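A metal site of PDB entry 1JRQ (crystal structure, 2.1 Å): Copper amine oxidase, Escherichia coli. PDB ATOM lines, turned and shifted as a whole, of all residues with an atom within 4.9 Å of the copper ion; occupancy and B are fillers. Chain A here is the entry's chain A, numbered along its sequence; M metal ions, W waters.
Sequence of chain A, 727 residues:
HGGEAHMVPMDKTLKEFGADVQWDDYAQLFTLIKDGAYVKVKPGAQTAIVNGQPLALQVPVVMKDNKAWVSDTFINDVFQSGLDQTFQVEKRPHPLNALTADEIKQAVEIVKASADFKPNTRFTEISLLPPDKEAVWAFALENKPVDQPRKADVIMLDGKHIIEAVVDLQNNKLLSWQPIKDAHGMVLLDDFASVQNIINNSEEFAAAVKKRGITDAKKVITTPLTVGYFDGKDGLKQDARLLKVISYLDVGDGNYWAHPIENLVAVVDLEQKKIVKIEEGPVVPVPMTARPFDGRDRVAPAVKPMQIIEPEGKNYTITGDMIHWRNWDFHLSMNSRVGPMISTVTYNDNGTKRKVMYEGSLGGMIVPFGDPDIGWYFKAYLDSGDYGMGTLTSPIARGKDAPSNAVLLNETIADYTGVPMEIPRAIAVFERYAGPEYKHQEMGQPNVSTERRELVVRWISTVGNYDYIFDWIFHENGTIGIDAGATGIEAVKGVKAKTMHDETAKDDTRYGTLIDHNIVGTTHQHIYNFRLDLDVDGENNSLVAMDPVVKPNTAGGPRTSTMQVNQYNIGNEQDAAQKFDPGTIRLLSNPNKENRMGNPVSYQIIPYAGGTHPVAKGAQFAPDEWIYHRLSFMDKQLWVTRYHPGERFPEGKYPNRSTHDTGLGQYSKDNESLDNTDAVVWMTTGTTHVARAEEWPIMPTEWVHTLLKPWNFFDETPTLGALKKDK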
ATOM      1  N   HIS A 524     -13.815  26.155  -9.272  1.00  0.00           N
ATOM      2  CA  HIS A 524     -13.215  24.868  -8.951  1.00  0.00           C
ATOM      3  C   HIS A 524     -11.729  24.967  -9.313  1.00  0.00           C
ATOM      4  O   HIS A 524     -11.287  26.017  -9.770  1.00  0.00           O
ATOM      5  CB  HIS A 524     -13.850  23.760  -9.820  1.00  0.00           C
ATOM      6  CG  HIS A 524     -13.799  24.188 -11.263  1.00  0.00           C
ATOM      7  ND1 HIS A 524     -14.723  25.063 -11.809  1.00  0.00           N
ATOM      8  CD2 HIS A 524     -12.897  23.832 -12.202  1.00  0.00           C
ATOM      9  CE1 HIS A 524     -14.442  25.256 -13.081  1.00  0.00           C
ATOM     10  NE2 HIS A 524     -13.375  24.526 -13.269  1.00  0.00           N
ATOM     11  N   HIS A 526      -8.199  22.763 -11.087  1.00  0.00           N
ATOM     12  CA  HIS A 526      -7.783  21.675 -11.968  1.00  0.00           C
ATOM     13  C   HIS A 526      -6.399  21.335 -11.401  1.00  0.00           C
ATOM     14  O   HIS A 526      -5.478  22.156 -11.511  1.00  0.00           O
ATOM     15  CB  HIS A 526      -7.658  22.059 -13.435  1.00  0.00           C
ATOM     16  CG  HIS A 526      -9.003  22.197 -14.062  1.00  0.00           C
ATOM     17  ND1 HIS A 526      -9.749  21.117 -14.475  1.00  0.00           N
ATOM     18  CD2 HIS A 526      -9.699  23.320 -14.346  1.00  0.00           C
ATOM     19  CE1 HIS A 526     -10.894  21.506 -15.015  1.00  0.00           C
ATOM     20  NE2 HIS A 526     -10.846  22.819 -14.923  1.00  0.00           N
ATOM     21  N   HIS A 613      -4.676  30.222 -17.169  1.00  0.00           N
ATOM     22  CA  HIS A 613      -5.767  30.412 -16.208  1.00  0.00           C
ATOM     23  C   HIS A 613      -4.998  30.740 -14.918  1.00  0.00           C
ATOM     24  O   HIS A 613      -3.813  30.450 -14.736  1.00  0.00           O
ATOM     25  CB  HIS A 613      -6.550  29.133 -15.966  1.00  0.00           C
ATOM     26  CG  HIS A 613      -7.920  29.062 -16.572  1.00  0.00           C
ATOM     27  ND1 HIS A 613      -8.645  27.890 -16.624  1.00  0.00           N
ATOM     28  CD2 HIS A 613      -8.683  30.027 -17.134  1.00  0.00           C
ATOM     29  CE1 HIS A 613      -9.800  28.133 -17.209  1.00  0.00           C
ATOM     30  NE2 HIS A 613      -9.858  29.413 -17.527  1.00  0.00           N
ATOM     31  N   HIS A 689     -10.023  27.911 -11.323  1.00  0.00           N
ATOM     32  CA  HIS A 689     -10.854  28.463 -12.383  1.00  0.00           C
ATOM     33  C   HIS A 689     -12.063  29.288 -12.011  1.00  0.00           C
ATOM     34  O   HIS A 689     -13.010  28.803 -11.402  1.00  0.00           O
ATOM     35  CB  HIS A 689     -11.268  27.254 -13.252  1.00  0.00           C
ATOM     36  CG  HIS A 689     -11.981  27.665 -14.505  1.00  0.00           C
ATOM     37  ND1 HIS A 689     -12.534  26.761 -15.363  1.00  0.00           N
ATOM     38  CD2 HIS A 689     -12.279  28.829 -15.117  1.00  0.00           C
ATOM     39  CE1 HIS A 689     -13.122  27.252 -16.429  1.00  0.00           C
ATOM     40  NE2 HIS A 689     -12.970  28.547 -16.268  1.00  0.00           N
ATOM     41  N   MET A 699     -15.597  25.700 -23.717  1.00  0.00           N
ATOM     42  CA  MET A 699     -14.400  26.411 -23.283  1.00  0.00           C
ATOM     43  C   MET A 699     -13.150  26.384 -24.136  1.00  0.00           C
ATOM     44  O   MET A 699     -12.630  25.308 -24.426  1.00  0.00           O
ATOM     45  CB  MET A 699     -13.987  25.892 -21.875  1.00  0.00           C
ATOM     46  CG  MET A 699     -12.877  26.709 -21.223  1.00  0.00           C
ATOM     47  SD  MET A 699     -12.225  26.384 -19.571  1.00  0.00           S
ATOM     48  CE  MET A 699     -10.824  25.317 -19.941  1.00  0.00           C
HETATM   49 CU    CU M   1     -12.112  24.560 -15.166  1.00  0.00          CU
HETATM   50  O   HOH W   1     -14.074  23.306 -16.452  1.00  0.00           O
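Of the 5 residues printed, 3 come within 4 Å of the copper ion.
The copper ion is bound by a ring nitrogen (NE2) of His 526 (2.2 Å), a ring nitrogen (ND1) of His 689 (2.2 Å) and a ring nitrogen (NE2) of His 524 (2.3 Å). Slightly farther from the copper ion lies water W1 (2.7 Å).
NE2 of His 689 sits close to NE2 of His 613 (3.5 Å).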
